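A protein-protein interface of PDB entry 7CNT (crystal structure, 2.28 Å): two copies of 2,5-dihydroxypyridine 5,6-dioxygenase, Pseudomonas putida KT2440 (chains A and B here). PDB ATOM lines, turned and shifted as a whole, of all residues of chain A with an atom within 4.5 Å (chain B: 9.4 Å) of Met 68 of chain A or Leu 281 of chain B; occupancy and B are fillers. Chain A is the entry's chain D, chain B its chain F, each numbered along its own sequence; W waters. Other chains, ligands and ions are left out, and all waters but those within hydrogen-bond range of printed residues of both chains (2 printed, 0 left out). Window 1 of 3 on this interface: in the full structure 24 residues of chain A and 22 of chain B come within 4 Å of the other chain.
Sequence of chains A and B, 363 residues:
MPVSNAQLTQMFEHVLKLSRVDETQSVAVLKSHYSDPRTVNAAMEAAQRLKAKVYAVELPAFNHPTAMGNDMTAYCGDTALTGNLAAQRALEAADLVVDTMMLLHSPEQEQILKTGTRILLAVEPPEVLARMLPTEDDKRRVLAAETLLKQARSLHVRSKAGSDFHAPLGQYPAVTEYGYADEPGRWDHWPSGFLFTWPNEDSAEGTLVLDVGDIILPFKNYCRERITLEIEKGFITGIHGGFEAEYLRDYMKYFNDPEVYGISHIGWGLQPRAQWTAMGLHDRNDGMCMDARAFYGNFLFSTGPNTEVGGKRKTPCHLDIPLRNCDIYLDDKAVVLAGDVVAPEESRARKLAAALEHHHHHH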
ATOM      1  N   THR A  66      -5.309 -15.006 -20.712  1.00  0.00           N
ATOM      2  CA  THR A  66      -5.330 -16.322 -21.315  1.00  0.00           C
ATOM      3  C   THR A  66      -6.734 -16.801 -21.699  1.00  0.00           C
ATOM      4  O   THR A  66      -6.862 -17.830 -22.352  1.00  0.00           O
ATOM      5  CB  THR A  66      -4.713 -17.365 -20.350  1.00  0.00           C
ATOM      6  OG1 THR A  66      -5.472 -17.404 -19.135  1.00  0.00           O
ATOM      7  CG2 THR A  66      -3.233 -17.030 -20.021  1.00  0.00           C
ATOM      8  N   ALA A  67      -7.791 -16.099 -21.298  1.00  0.00           N
ATOM      9  CA  ALA A  67      -9.150 -16.552 -21.663  1.00  0.00           C
ATOM     10  C   ALA A  67      -9.405 -16.515 -23.194  1.00  0.00           C
ATOM     11  O   ALA A  67      -8.949 -15.593 -23.898  1.00  0.00           O
ATOM     12  CB  ALA A  67     -10.209 -15.754 -20.921  1.00  0.00           C
ATOM     13  N   MET A  68     -10.106 -17.535 -23.697  1.00  0.00           N
ATOM     14  CA  MET A  68     -10.445 -17.612 -25.128  1.00  0.00           C
ATOM     15  C   MET A  68     -11.936 -17.491 -25.377  1.00  0.00           C
ATOM     16  O   MET A  68     -12.735 -17.721 -24.477  1.00  0.00           O
ATOM     17  CB  MET A  68      -9.939 -18.904 -25.752  1.00  0.00           C
ATOM     18  CG  MET A  68      -8.619 -19.399 -25.172  1.00  0.00           C
ATOM     19  SD  MET A  68      -7.901 -20.671 -26.484  1.00  0.00           S
ATOM     20  CE  MET A  68      -8.137 -22.206 -25.290  1.00  0.00           C
ATOM     21  N   GLY A  69     -12.297 -17.128 -26.616  1.00  0.00           N
ATOM     22  CA  GLY A  69     -13.677 -16.782 -27.003  1.00  0.00           C
ATOM     23  C   GLY A  69     -14.256 -15.544 -26.307  1.00  0.00           C
ATOM     24  O   GLY A  69     -13.543 -14.817 -25.623  1.00  0.00           O
ATOM     25  N   ASN A  70     -15.560 -15.313 -26.472  1.00  0.00           N
ATOM     26  CA  ASN A  70     -16.239 -14.159 -25.852  1.00  0.00           C
ATOM     27  C   ASN A  70     -17.239 -14.505 -24.739  1.00  0.00           C
ATOM     28  O   ASN A  70     -17.814 -13.601 -24.112  1.00  0.00           O
ATOM     29  CB  ASN A  70     -16.942 -13.328 -26.926  1.00  0.00           C
ATOM     30  CG  ASN A  70     -15.958 -12.641 -27.863  1.00  0.00           C
ATOM     31  OD1 ASN A  70     -15.325 -11.650 -27.493  1.00  0.00           O
ATOM     32  ND2 ASN A  70     -15.825 -13.164 -29.081  1.00  0.00           N
ATOM     33  N   ALA A  74     -16.630 -19.039 -19.500  1.00  0.00           N
ATOM     34  CA  ALA A  74     -15.514 -19.913 -19.916  1.00  0.00           C
ATOM     35  C   ALA A  74     -14.295 -19.868 -19.006  1.00  0.00           C
ATOM     36  O   ALA A  74     -13.572 -20.867 -18.891  1.00  0.00           O
ATOM     37  CB  ALA A  74     -15.074 -19.564 -21.335  1.00  0.00           C
ATOM     38  N   PRO A 218     -18.679 -23.910 -22.906  1.00  0.00           N
ATOM     39  CA  PRO A 218     -19.013 -22.870 -23.860  1.00  0.00           C
ATOM     40  C   PRO A 218     -18.692 -23.155 -25.318  1.00  0.00           C
ATOM     41  O   PRO A 218     -18.765 -22.243 -26.099  1.00  0.00           O
ATOM     42  CB  PRO A 218     -18.147 -21.722 -23.393  1.00  0.00           C
ATOM     43  CG  PRO A 218     -16.923 -22.394 -22.859  1.00  0.00           C
ATOM     44  CD  PRO A 218     -17.345 -23.706 -22.308  1.00  0.00           C
ATOM     45  N   PHE A 219     -18.372 -24.392 -25.693  1.00  0.00           N
ATOM     46  CA  PHE A 219     -18.129 -24.713 -27.103  1.00  0.00           C
ATOM     47  C   PHE A 219     -19.378 -24.442 -27.997  1.00  0.00           C
ATOM     48  O   PHE A 219     -19.272 -24.141 -29.180  1.00  0.00           O
ATOM     49  CB  PHE A 219     -17.784 -26.182 -27.278  1.00  0.00           C
ATOM     50  CG  PHE A 219     -16.682 -26.680 -26.415  1.00  0.00           C
ATOM     51  CD1 PHE A 219     -15.887 -25.821 -25.656  1.00  0.00           C
ATOM     52  CD2 PHE A 219     -16.399 -28.039 -26.421  1.00  0.00           C
ATOM     53  CE1 PHE A 219     -14.861 -26.316 -24.884  1.00  0.00           C
ATOM     54  CE2 PHE A 219     -15.358 -28.536 -25.666  1.00  0.00           C
ATOM     55  CZ  PHE A 219     -14.587 -27.669 -24.900  1.00  0.00           C
ATOM     56  N   TYR A 247     -10.727 -32.775 -28.814  1.00  0.00           N
ATOM     57  CA  TYR A 247     -10.815 -31.343 -28.725  1.00  0.00           C
ATOM     58  C   TYR A 247     -11.027 -31.006 -27.245  1.00  0.00           C
ATOM     59  O   TYR A 247     -10.400 -30.068 -26.701  1.00  0.00           O
ATOM     60  CB  TYR A 247     -11.919 -30.810 -29.673  1.00  0.00           C
ATOM     61  CG  TYR A 247     -12.145 -29.338 -29.618  1.00  0.00           C
ATOM     62  CD1 TYR A 247     -12.864 -28.756 -28.552  1.00  0.00           C
ATOM     63  CD2 TYR A 247     -11.646 -28.507 -30.597  1.00  0.00           C
ATOM     64  CE1 TYR A 247     -13.067 -27.383 -28.489  1.00  0.00           C
ATOM     65  CE2 TYR A 247     -11.848 -27.120 -30.536  1.00  0.00           C
ATOM     66  CZ  TYR A 247     -12.567 -26.575 -29.496  1.00  0.00           C
ATOM     67  OH  TYR A 247     -12.764 -25.212 -29.447  1.00  0.00           O
ATOM     68  N   TYR A 251      -8.527 -28.966 -24.807  1.00  0.00           N
ATOM     69  CA  TYR A 251      -9.008 -27.722 -24.262  1.00  0.00           C
ATOM     70  C   TYR A 251      -8.762 -27.671 -22.751  1.00  0.00           C
ATOM     71  O   TYR A 251      -8.378 -26.630 -22.213  1.00  0.00           O
ATOM     72  CB  TYR A 251     -10.495 -27.515 -24.577  1.00  0.00           C
ATOM     73  CG  TYR A 251     -11.082 -26.269 -23.914  1.00  0.00           C
ATOM     74  CD1 TYR A 251     -10.769 -25.001 -24.368  1.00  0.00           C
ATOM     75  CD2 TYR A 251     -11.903 -26.381 -22.789  1.00  0.00           C
ATOM     76  CE1 TYR A 251     -11.301 -23.853 -23.744  1.00  0.00           C
ATOM     77  CE2 TYR A 251     -12.443 -25.249 -22.160  1.00  0.00           C
ATOM     78  CZ  TYR A 251     -12.141 -23.988 -22.634  1.00  0.00           C
ATOM     79  OH  TYR A 251     -12.686 -22.894 -21.989  1.00  0.00           O
ATOM     80  N   TYR A 254      -4.882 -27.169 -21.701  1.00  0.00           N
ATOM     81  CA  TYR A 254      -4.311 -25.834 -21.892  1.00  0.00           C
ATOM     82  C   TYR A 254      -4.277 -25.054 -20.602  1.00  0.00           C
ATOM     83  O   TYR A 254      -3.401 -24.207 -20.393  1.00  0.00           O
ATOM     84  CB  TYR A 254      -5.136 -25.084 -22.907  1.00  0.00           C
ATOM     85  CG  TYR A 254      -5.018 -23.569 -22.938  1.00  0.00           C
ATOM     86  CD1 TYR A 254      -3.963 -22.955 -23.624  1.00  0.00           C
ATOM     87  CD2 TYR A 254      -6.012 -22.749 -22.342  1.00  0.00           C
ATOM     88  CE1 TYR A 254      -3.875 -21.582 -23.706  1.00  0.00           C
ATOM     89  CE2 TYR A 254      -5.938 -21.369 -22.417  1.00  0.00           C
ATOM     90  CZ  TYR A 254      -4.868 -20.791 -23.108  1.00  0.00           C
ATOM     91  OH  TYR A 254      -4.771 -19.433 -23.213  1.00  0.00           O
ATOM     92  N   ARG A 284     -22.571 -18.111 -31.755  1.00  0.00           N
ATOM     93  CA  ARG A 284     -21.764 -18.191 -30.533  1.00  0.00           C
ATOM     94  C   ARG A 284     -21.786 -16.904 -29.690  1.00  0.00           C
ATOM     95  O   ARG A 284     -21.909 -16.962 -28.469  1.00  0.00           O
ATOM     96  CB  ARG A 284     -20.307 -18.502 -30.902  1.00  0.00           C
ATOM     97  CG  ARG A 284     -20.101 -19.886 -31.501  1.00  0.00           C
ATOM     98  CD  ARG A 284     -18.786 -20.494 -31.044  1.00  0.00           C
ATOM     99  NE  ARG A 284     -18.745 -21.929 -31.291  1.00  0.00           N
ATOM    100  CZ  ARG A 284     -18.478 -22.490 -32.469  1.00  0.00           C
ATOM    101  NH1 ARG A 284     -18.223 -21.732 -33.533  1.00  0.00           N
ATOM    102  NH2 ARG A 284     -18.460 -23.817 -32.574  1.00  0.00           N
ATOM    103  N   PRO B   2     -13.587  -9.121 -20.899  1.00  0.00           N
ATOM    104  CA  PRO B   2     -13.140  -8.416 -22.085  1.00  0.00           C
ATOM    105  C   PRO B   2     -12.232  -7.258 -21.770  1.00  0.00           C
ATOM    106  O   PRO B   2     -12.032  -6.943 -20.612  1.00  0.00           O
ATOM    107  CB  PRO B   2     -14.440  -7.885 -22.711  1.00  0.00           C
ATOM    108  CG  PRO B   2     -15.510  -8.810 -22.244  1.00  0.00           C
ATOM    109  CD  PRO B   2     -15.052  -9.300 -20.884  1.00  0.00           C
ATOM    110  N   GLU B 127      -9.589  -8.923 -27.402  1.00  0.00           N
ATOM    111  CA  GLU B 127      -9.261 -10.102 -26.570  1.00  0.00           C
ATOM    112  C   GLU B 127      -8.157 -10.971 -27.198  1.00  0.00           C
ATOM    113  O   GLU B 127      -7.292 -11.517 -26.510  1.00  0.00           O
ATOM    114  CB  GLU B 127     -10.503 -10.954 -26.302  1.00  0.00           C
ATOM    115  CG  GLU B 127     -11.514 -10.202 -25.456  1.00  0.00           C
ATOM    116  CD  GLU B 127     -12.088  -8.972 -26.172  1.00  0.00           C
ATOM    117  OE1 GLU B 127     -12.252  -9.053 -27.434  1.00  0.00           O
ATOM    118  OE2 GLU B 127     -12.353  -7.928 -25.486  1.00  0.00           O
ATOM    119  N   VAL B 128      -8.212 -11.097 -28.511  1.00  0.00           N
ATOM    120  CA  VAL B 128      -7.256 -11.888 -29.254  1.00  0.00           C
ATOM    121  C   VAL B 128      -5.949 -11.122 -29.216  1.00  0.00           C
ATOM    122  O   VAL B 128      -4.911 -11.719 -29.036  1.00  0.00           O
ATOM    123  CB  VAL B 128      -7.729 -12.100 -30.727  1.00  0.00           C
ATOM    124  CG1 VAL B 128      -6.700 -12.829 -31.555  1.00  0.00           C
ATOM    125  CG2 VAL B 128      -9.042 -12.875 -30.798  1.00  0.00           C
ATOM    126  N   ARG B 131      -4.419 -11.685 -25.622  1.00  0.00           N
ATOM    127  CA  ARG B 131      -3.975 -13.035 -25.433  1.00  0.00           C
ATOM    128  C   ARG B 131      -2.607 -13.321 -26.117  1.00  0.00           C
ATOM    129  O   ARG B 131      -1.802 -14.165 -25.607  1.00  0.00           O
ATOM    130  CB  ARG B 131      -5.065 -14.005 -25.890  1.00  0.00           C
ATOM    131  CG  ARG B 131      -4.716 -15.471 -25.640  1.00  0.00           C
ATOM    132  CD  ARG B 131      -5.931 -16.370 -25.533  1.00  0.00           C
ATOM    133  NE  ARG B 131      -6.846 -16.240 -26.676  1.00  0.00           N
ATOM    134  CZ  ARG B 131      -6.590 -16.685 -27.902  1.00  0.00           C
ATOM    135  NH1 ARG B 131      -5.419 -17.270 -28.191  1.00  0.00           N
ATOM    136  NH2 ARG B 131      -7.488 -16.520 -28.866  1.00  0.00           N
ATOM    137  N   MET B 132      -2.356 -12.593 -27.227  1.00  0.00           N
ATOM    138  CA  MET B 132      -1.172 -12.784 -28.070  1.00  0.00           C
ATOM    139  C   MET B 132      -0.363 -11.515 -28.184  1.00  0.00           C
ATOM    140  O   MET B 132       0.195 -11.200 -29.249  1.00  0.00           O
ATOM    141  CB  MET B 132      -1.617 -13.346 -29.405  1.00  0.00           C
ATOM    142  CG  MET B 132      -1.895 -14.856 -29.289  1.00  0.00           C
ATOM    143  SD  MET B 132      -2.332 -15.574 -31.084  1.00  0.00           S
ATOM    144  CE  MET B 132      -4.170 -14.956 -31.263  1.00  0.00           C
ATOM    145  N   LYS B 220     -13.107 -21.887 -41.874  1.00  0.00           N
ATOM    146  CA  LYS B 220     -13.102 -21.947 -40.407  1.00  0.00           C
ATOM    147  C   LYS B 220     -13.794 -23.145 -39.795  1.00  0.00           C
ATOM    148  O   LYS B 220     -14.395 -23.038 -38.731  1.00  0.00           O
ATOM    149  CB  LYS B 220     -13.607 -20.647 -39.787  1.00  0.00           C
ATOM    150  CG  LYS B 220     -12.792 -19.453 -40.273  1.00  0.00           C
ATOM    151  CD  LYS B 220     -13.233 -18.154 -39.654  1.00  0.00           C
ATOM    152  CE  LYS B 220     -12.433 -16.998 -40.237  1.00  0.00           C
ATOM    153  NZ  LYS B 220     -13.278 -16.018 -40.957  1.00  0.00           N
ATOM    154  N   TYR B 222     -13.256 -27.288 -38.457  1.00  0.00           N
ATOM    155  CA  TYR B 222     -12.452 -28.452 -38.139  1.00  0.00           C
ATOM    156  C   TYR B 222     -12.908 -29.546 -39.078  1.00  0.00           C
ATOM    157  O   TYR B 222     -14.057 -29.956 -38.992  1.00  0.00           O
ATOM    158  CB  TYR B 222     -12.660 -28.872 -36.672  1.00  0.00           C
ATOM    159  CG  TYR B 222     -12.131 -27.845 -35.699  1.00  0.00           C
ATOM    160  CD1 TYR B 222     -10.761 -27.722 -35.468  1.00  0.00           C
ATOM    161  CD2 TYR B 222     -12.972 -26.971 -35.055  1.00  0.00           C
ATOM    162  CE1 TYR B 222     -10.271 -26.788 -34.573  1.00  0.00           C
ATOM    163  CE2 TYR B 222     -12.494 -26.020 -34.177  1.00  0.00           C
ATOM    164  CZ  TYR B 222     -11.140 -25.946 -33.930  1.00  0.00           C
ATOM    165  OH  TYR B 222     -10.647 -24.976 -33.091  1.00  0.00           O
ATOM    166  N   PRO B 272       3.099 -20.186 -29.129  1.00  0.00           N
ATOM    167  CA  PRO B 272       2.505 -21.072 -28.163  1.00  0.00           C
ATOM    168  C   PRO B 272       1.275 -20.505 -27.444  1.00  0.00           C
ATOM    169  O   PRO B 272       0.598 -21.231 -26.775  1.00  0.00           O
ATOM    170  CB  PRO B 272       3.701 -21.302 -27.184  1.00  0.00           C
ATOM    171  CG  PRO B 272       4.360 -19.983 -27.175  1.00  0.00           C
ATOM    172  CD  PRO B 272       4.397 -19.680 -28.646  1.00  0.00           C
ATOM    173  N   ARG B 273       1.034 -19.208 -27.519  1.00  0.00           N
ATOM    174  CA  ARG B 273      -0.140 -18.621 -26.882  1.00  0.00           C
ATOM    175  C   ARG B 273      -1.381 -18.684 -27.831  1.00  0.00           C
ATOM    176  O   ARG B 273      -2.543 -18.452 -27.430  1.00  0.00           O
ATOM    177  CB  ARG B 273       0.177 -17.186 -26.415  1.00  0.00           C
ATOM    178  CG  ARG B 273       1.046 -17.141 -25.133  1.00  0.00           C
ATOM    179  CD  ARG B 273       1.424 -15.724 -24.723  1.00  0.00           C
ATOM    180  NE  ARG B 273       2.295 -15.108 -25.715  1.00  0.00           N
ATOM    181  CZ  ARG B 273       2.343 -13.798 -25.951  1.00  0.00           C
ATOM    182  NH1 ARG B 273       1.578 -12.962 -25.271  1.00  0.00           N
ATOM    183  NH2 ARG B 273       3.152 -13.315 -26.879  1.00  0.00           N
ATOM    184  N   ALA B 274      -1.116 -19.038 -29.080  1.00  0.00           N
ATOM    185  CA  ALA B 274      -2.164 -19.293 -30.045  1.00  0.00           C
ATOM    186  C   ALA B 274      -2.512 -20.726 -29.792  1.00  0.00           C
ATOM    187  O   ALA B 274      -1.630 -21.539 -29.460  1.00  0.00           O
ATOM    188  CB  ALA B 274      -1.655 -19.117 -31.467  1.00  0.00           C
ATOM    189  N   GLN B 275      -3.789 -21.033 -29.948  1.00  0.00           N
ATOM    190  CA  GLN B 275      -4.340 -22.356 -29.654  1.00  0.00           C
ATOM    191  C   GLN B 275      -5.232 -22.840 -30.792  1.00  0.00           C
ATOM    192  O   GLN B 275      -6.085 -22.106 -31.298  1.00  0.00           O
ATOM    193  CB  GLN B 275      -5.192 -22.321 -28.379  1.00  0.00           C
ATOM    194  CG  GLN B 275      -4.410 -22.068 -27.101  1.00  0.00           C
ATOM    195  CD  GLN B 275      -3.473 -23.213 -26.715  1.00  0.00           C
ATOM    196  OE1 GLN B 275      -3.860 -24.405 -26.659  1.00  0.00           O
ATOM    197  NE2 GLN B 275      -2.248 -22.862 -26.434  1.00  0.00           N
ATOM    198  N   TRP B 276      -5.011 -24.101 -31.142  1.00  0.00           N
ATOM    199  CA  TRP B 276      -5.684 -24.779 -32.185  1.00  0.00           C
ATOM    200  C   TRP B 276      -7.164 -24.861 -31.843  1.00  0.00           C
ATOM    201  O   TRP B 276      -7.942 -25.012 -32.733  1.00  0.00           O
ATOM    202  CB  TRP B 276      -5.078 -26.200 -32.343  1.00  0.00           C
ATOM    203  CG  TRP B 276      -5.940 -27.171 -33.061  1.00  0.00           C
ATOM    204  CD1 TRP B 276      -6.144 -27.249 -34.415  1.00  0.00           C
ATOM    205  CD2 TRP B 276      -6.748 -28.203 -32.473  1.00  0.00           C
ATOM    206  NE1 TRP B 276      -7.020 -28.284 -34.707  1.00  0.00           N
ATOM    207  CE2 TRP B 276      -7.405 -28.879 -33.534  1.00  0.00           C
ATOM    208  CE3 TRP B 276      -6.956 -28.641 -31.163  1.00  0.00           C
ATOM    209  CZ2 TRP B 276      -8.284 -29.944 -33.316  1.00  0.00           C
ATOM    210  CZ3 TRP B 276      -7.839 -29.713 -30.942  1.00  0.00           C
ATOM    211  CH2 TRP B 276      -8.479 -30.357 -32.017  1.00  0.00           C
ATOM    212  N   THR B 277      -7.521 -24.818 -30.556  1.00  0.00           N
ATOM    213  CA  THR B 277      -8.910 -24.978 -30.112  1.00  0.00           C
ATOM    214  C   THR B 277      -9.655 -23.639 -30.103  1.00  0.00           C
ATOM    215  O   THR B 277     -10.849 -23.597 -29.829  1.00  0.00           O
ATOM    216  CB  THR B 277      -9.013 -25.548 -28.662  1.00  0.00           C
ATOM    217  OG1 THR B 277      -8.316 -24.684 -27.787  1.00  0.00           O
ATOM    218  CG2 THR B 277      -8.446 -26.970 -28.522  1.00  0.00           C
ATOM    219  N   ALA B 278      -8.952 -22.540 -30.338  1.00  0.00           N
ATOM    220  CA  ALA B 278      -9.576 -21.239 -30.208  1.00  0.00           C
ATOM    221  C   ALA B 278     -10.669 -21.036 -31.256  1.00  0.00           C
ATOM    222  O   ALA B 278     -11.647 -20.374 -30.993  1.00  0.00           O
ATOM    223  CB  ALA B 278      -8.540 -20.133 -30.310  1.00  0.00           C
ATOM    224  N   MET B 279     -10.506 -21.600 -32.436  1.00  0.00           N
ATOM    225  CA  MET B 279     -11.399 -21.258 -33.522  1.00  0.00           C
ATOM    226  C   MET B 279     -12.816 -21.658 -33.184  1.00  0.00           C
ATOM    227  O   MET B 279     -13.730 -20.908 -33.480  1.00  0.00           O
ATOM    228  CB  MET B 279     -10.944 -21.932 -34.788  1.00  0.00           C
ATOM    229  CG  MET B 279     -11.831 -21.580 -35.974  1.00  0.00           C
ATOM    230  SD  MET B 279     -10.970 -22.291 -37.604  1.00  0.00           S
ATOM    231  CE  MET B 279     -11.327 -24.217 -37.397  1.00  0.00           C
ATOM    232  N   GLY B 280     -12.999 -22.786 -32.497  1.00  0.00           N
ATOM    233  CA  GLY B 280     -14.322 -23.267 -32.072  1.00  0.00           C
ATOM    234  C   GLY B 280     -14.983 -22.535 -30.900  1.00  0.00           C
ATOM    235  O   GLY B 280     -15.984 -23.035 -30.348  1.00  0.00           O
ATOM    236  N   LEU B 281     -14.422 -21.379 -30.503  1.00  0.00           N
ATOM    237  CA  LEU B 281     -15.026 -20.513 -29.489  1.00  0.00           C
ATOM    238  C   LEU B 281     -15.464 -19.172 -30.059  1.00  0.00           C
ATOM    239  O   LEU B 281     -16.084 -18.366 -29.361  1.00  0.00           O
ATOM    240  CB  LEU B 281     -14.052 -20.303 -28.345  1.00  0.00           C
ATOM    241  CG  LEU B 281     -13.662 -21.651 -27.739  1.00  0.00           C
ATOM    242  CD1 LEU B 281     -12.319 -21.568 -27.042  1.00  0.00           C
ATOM    243  CD2 LEU B 281     -14.749 -22.125 -26.791  1.00  0.00           C
ATOM    244  N   HIS B 282     -15.171 -18.971 -31.346  1.00  0.00           N
ATOM    245  CA  HIS B 282     -15.422 -17.717 -32.038  1.00  0.00           C
ATOM    246  C   HIS B 282     -16.393 -17.920 -33.189  1.00  0.00           C
ATOM    247  O   HIS B 282     -16.562 -19.047 -33.679  1.00  0.00           O
ATOM    248  CB  HIS B 282     -14.110 -17.184 -32.624  1.00  0.00           C
ATOM    249  CG  HIS B 282     -13.180 -16.610 -31.606  1.00  0.00           C
ATOM    250  ND1 HIS B 282     -13.353 -15.349 -31.071  1.00  0.00           N
ATOM    251  CD2 HIS B 282     -12.057 -17.113 -31.039  1.00  0.00           C
ATOM    252  CE1 HIS B 282     -12.383 -15.103 -30.212  1.00  0.00           C
ATOM    253  NE2 HIS B 282     -11.584 -16.156 -30.174  1.00  0.00           N
ATOM    254  N   ASP B 283     -17.017 -16.820 -33.616  1.00  0.00           N
ATOM    255  CA  ASP B 283     -17.812 -16.788 -34.845  1.00  0.00           C
ATOM    256  C   ASP B 283     -16.923 -16.395 -36.013  1.00  0.00           C
ATOM    257  O   ASP B 283     -15.860 -15.805 -35.832  1.00  0.00           O
ATOM    258  CB  ASP B 283     -18.987 -15.801 -34.728  1.00  0.00           C
ATOM    259  CG  ASP B 283     -20.225 -16.412 -34.012  1.00  0.00           C
ATOM    260  OD1 ASP B 283     -20.650 -17.575 -34.322  1.00  0.00           O
ATOM    261  OD2 ASP B 283     -20.784 -15.701 -33.139  1.00  0.00           O
ATOM    262  N   ARG B 284     -17.369 -16.742 -37.216  1.00  0.00           N
ATOM    263  CA  ARG B 284     -16.612 -16.485 -38.441  1.00  0.00           C
ATOM    264  C   ARG B 284     -16.291 -14.994 -38.663  1.00  0.00           C
ATOM    265  O   ARG B 284     -15.209 -14.662 -39.135  1.00  0.00           O
ATOM    266  CB  ARG B 284     -17.361 -17.019 -39.662  1.00  0.00           C
ATOM    267  CG  ARG B 284     -17.579 -18.505 -39.637  1.00  0.00           C
ATOM    268  CD  ARG B 284     -17.845 -19.039 -41.033  1.00  0.00           C
ATOM    269  NE  ARG B 284     -17.904 -20.509 -41.034  1.00  0.00           N
ATOM    270  CZ  ARG B 284     -19.016 -21.250 -40.957  1.00  0.00           C
ATOM    271  NH1 ARG B 284     -20.229 -20.698 -40.889  1.00  0.00           N
ATOM    272  NH2 ARG B 284     -18.904 -22.572 -40.971  1.00  0.00           N
ATOM    273  N   ASP B 286     -15.785 -12.770 -36.435  1.00  0.00           N
ATOM    274  CA  ASP B 286     -14.971 -12.199 -35.336  1.00  0.00           C
ATOM    275  C   ASP B 286     -13.627 -11.682 -35.838  1.00  0.00           C
ATOM    276  O   ASP B 286     -13.179 -10.590 -35.455  1.00  0.00           O
ATOM    277  CB  ASP B 286     -14.779 -13.214 -34.218  1.00  0.00           C
ATOM    278  CG  ASP B 286     -16.076 -13.512 -33.484  1.00  0.00           C
ATOM    279  OD1 ASP B 286     -17.059 -12.776 -33.735  1.00  0.00           O
ATOM    280  OD2 ASP B 286     -16.120 -14.476 -32.669  1.00  0.00           O
ATOM    281  N   CYS B 289      -8.753 -15.489 -37.521  1.00  0.00           N
ATOM    282  CA  CYS B 289      -8.247 -16.662 -36.855  1.00  0.00           C
ATOM    283  C   CYS B 289      -6.706 -16.813 -36.960  1.00  0.00           C
ATOM    284  O   CYS B 289      -6.153 -17.827 -37.397  1.00  0.00           O
ATOM    285  CB  CYS B 289      -8.989 -17.931 -37.277  1.00  0.00           C
ATOM    286  SG  CYS B 289      -8.910 -19.148 -35.931  1.00  0.00           S
ATOM    287  N   ASP B 291      -5.039 -17.513 -34.480  1.00  0.00           N
ATOM    288  CA  ASP B 291      -4.760 -18.733 -33.690  1.00  0.00           C
ATOM    289  C   ASP B 291      -4.510 -19.977 -34.567  1.00  0.00           C
ATOM    290  O   ASP B 291      -3.697 -20.858 -34.242  1.00  0.00           O
ATOM    291  CB  ASP B 291      -5.912 -19.080 -32.760  1.00  0.00           C
ATOM    292  CG  ASP B 291      -5.902 -18.281 -31.490  1.00  0.00           C
ATOM    293  OD1 ASP B 291      -5.119 -18.649 -30.560  1.00  0.00           O
ATOM    294  OD2 ASP B 291      -6.674 -17.284 -31.394  1.00  0.00           O
HETATM  295  O   HOH W   1      -8.854 -14.667 -26.294  1.00  0.00           O
HETATM  296  O   HOH W   2      -9.984 -15.937 -28.279  1.00  0.00           O
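The side-chain hydroxyl (OH) of Tyr 247 of chain A lies within hydrogen-bond range of the backbone carbonyl oxygen (O) of Thr 277 of chain B (2.5 Å). NE of Arg 284 of chain A sits at hydrogen-bond distance from O of Gly 280 of chain B (3.1 Å). NH1 of Arg 284 of chain A sits at hydrogen-bond distance from O of His 282 of chain B (3.2 Å). OD1 of Asp 283 of chain B is in hydrogen-bond range of N of Arg 284 of chain A (3.3 Å).
The guanidinium group of Arg 131 of chain B lies within hydrogen-bond range of the backbone carbonyl oxygen of Arg 273 of chain B (3.2 Å). N of Met 279 of chain B lies within hydrogen-bond range of OH of Tyr 222 of chain B (3.4 Å). The backbone NH (N) of Asp 283 of chain B lies within hydrogen-bond range of the side-chain carboxylate (OD2) of Asp 286 of chain B (2.7 Å).
Among the printed residues, pairs that only touch across the chains: Thr 66 of chain A with Arg 131 of chain B (3.6 Å), Ala 67 of chain A with Arg 131 of chain B (3.5 Å), Met 68 of chain A with Arg 131 of chain B (3.9 Å), Met 68 of chain A with Gln 275 of chain B (3.7 Å), Met 68 of chain A with Thr 277 of chain B (3.5 Å), Met 68 of chain A with Ala 278 of chain B (3.9 Å), Met 68 of chain A with Leu 281 of chain B (3.8 Å), Gly 69 of chain A with Leu 281 of chain B (3.7 Å), Gly 69 of chain A with His 282 of chain B (3.8 Å), Asn 70 of chain A with His 282 of chain B (3.9 Å), Asn 70 of chain A with Asp 286 of chain B (3.8 Å), Phe 219 of chain A with Gly 280 of chain B (3.7 Å), Tyr 247 of chain A with Tyr 222 of chain B (3.5 Å), Tyr 247 of chain A with Trp 276 of chain B (3.9 Å), Tyr 247 of chain A with Gly 280 of chain B (3.6 Å), Tyr 254 of chain A with Gln 275 of chain B (3.1 Å) and Arg 284 of chain A with Leu 281 of chain B (3.7 Å).
Printed residues of chain B within 4 Å of Ala 67 of chain A: Arg 131. Tyr 251 of chain A touches none of the printed residues of chain B. Lys 220 of chain B touches none of the printed residues of chain A. Printed residues of chain A within 4 Å of Tyr 222 of chain B: Tyr 247. Of chain A, only Met 68 (3.8 Å), Gly 69 (3.7 Å) and Arg 284 (3.7 Å) come within 4 Å of Leu 281 of chain B. Printed residues of chain A within 4 Å of Asp 286 of chain B: Asn 70. The nearest printed residue of chain A that does not touch Leu 281 of chain B is Phe 219 of chain A (4.03 Å). The nearest printed residue of chain B that does not touch Thr 66 of chain A is Arg 273 of chain B (6.7 Å).
Printed residues of chain B that touch a printed residue of chain A: Arg 131, Tyr 222, Gln 275, Trp 276, Thr 277, Ala 278, Gly 280, Leu 281, His 282, Asp 283 and Asp 286. Hydrophobic or aromatic side chains of chain B that line the printed part of chain A: Tyr 222, Trp 276, Ala 278, Leu 281 and His 282. Among the printed residues, no Asp or Glu carboxylate lies within 4 Å of a Lys or Arg side-chain nitrogen of the other chain.
Position printed for both chains: 284.
Water W2 lies within hydrogen-bond range of a ring nitrogen (NE2) of His 282 of chain B (2.5 Å), the guanidinium group of Arg 131 of chain B (2.6 Å) and the backbone NH of Gly 69 of chain A (3.1 Å). Water W1 bridges the backbone carbonyl oxygen of Ala 67 of chain A (2.6 Å) and the guanidinium group of Arg 131 of chain B (2.6 Å).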
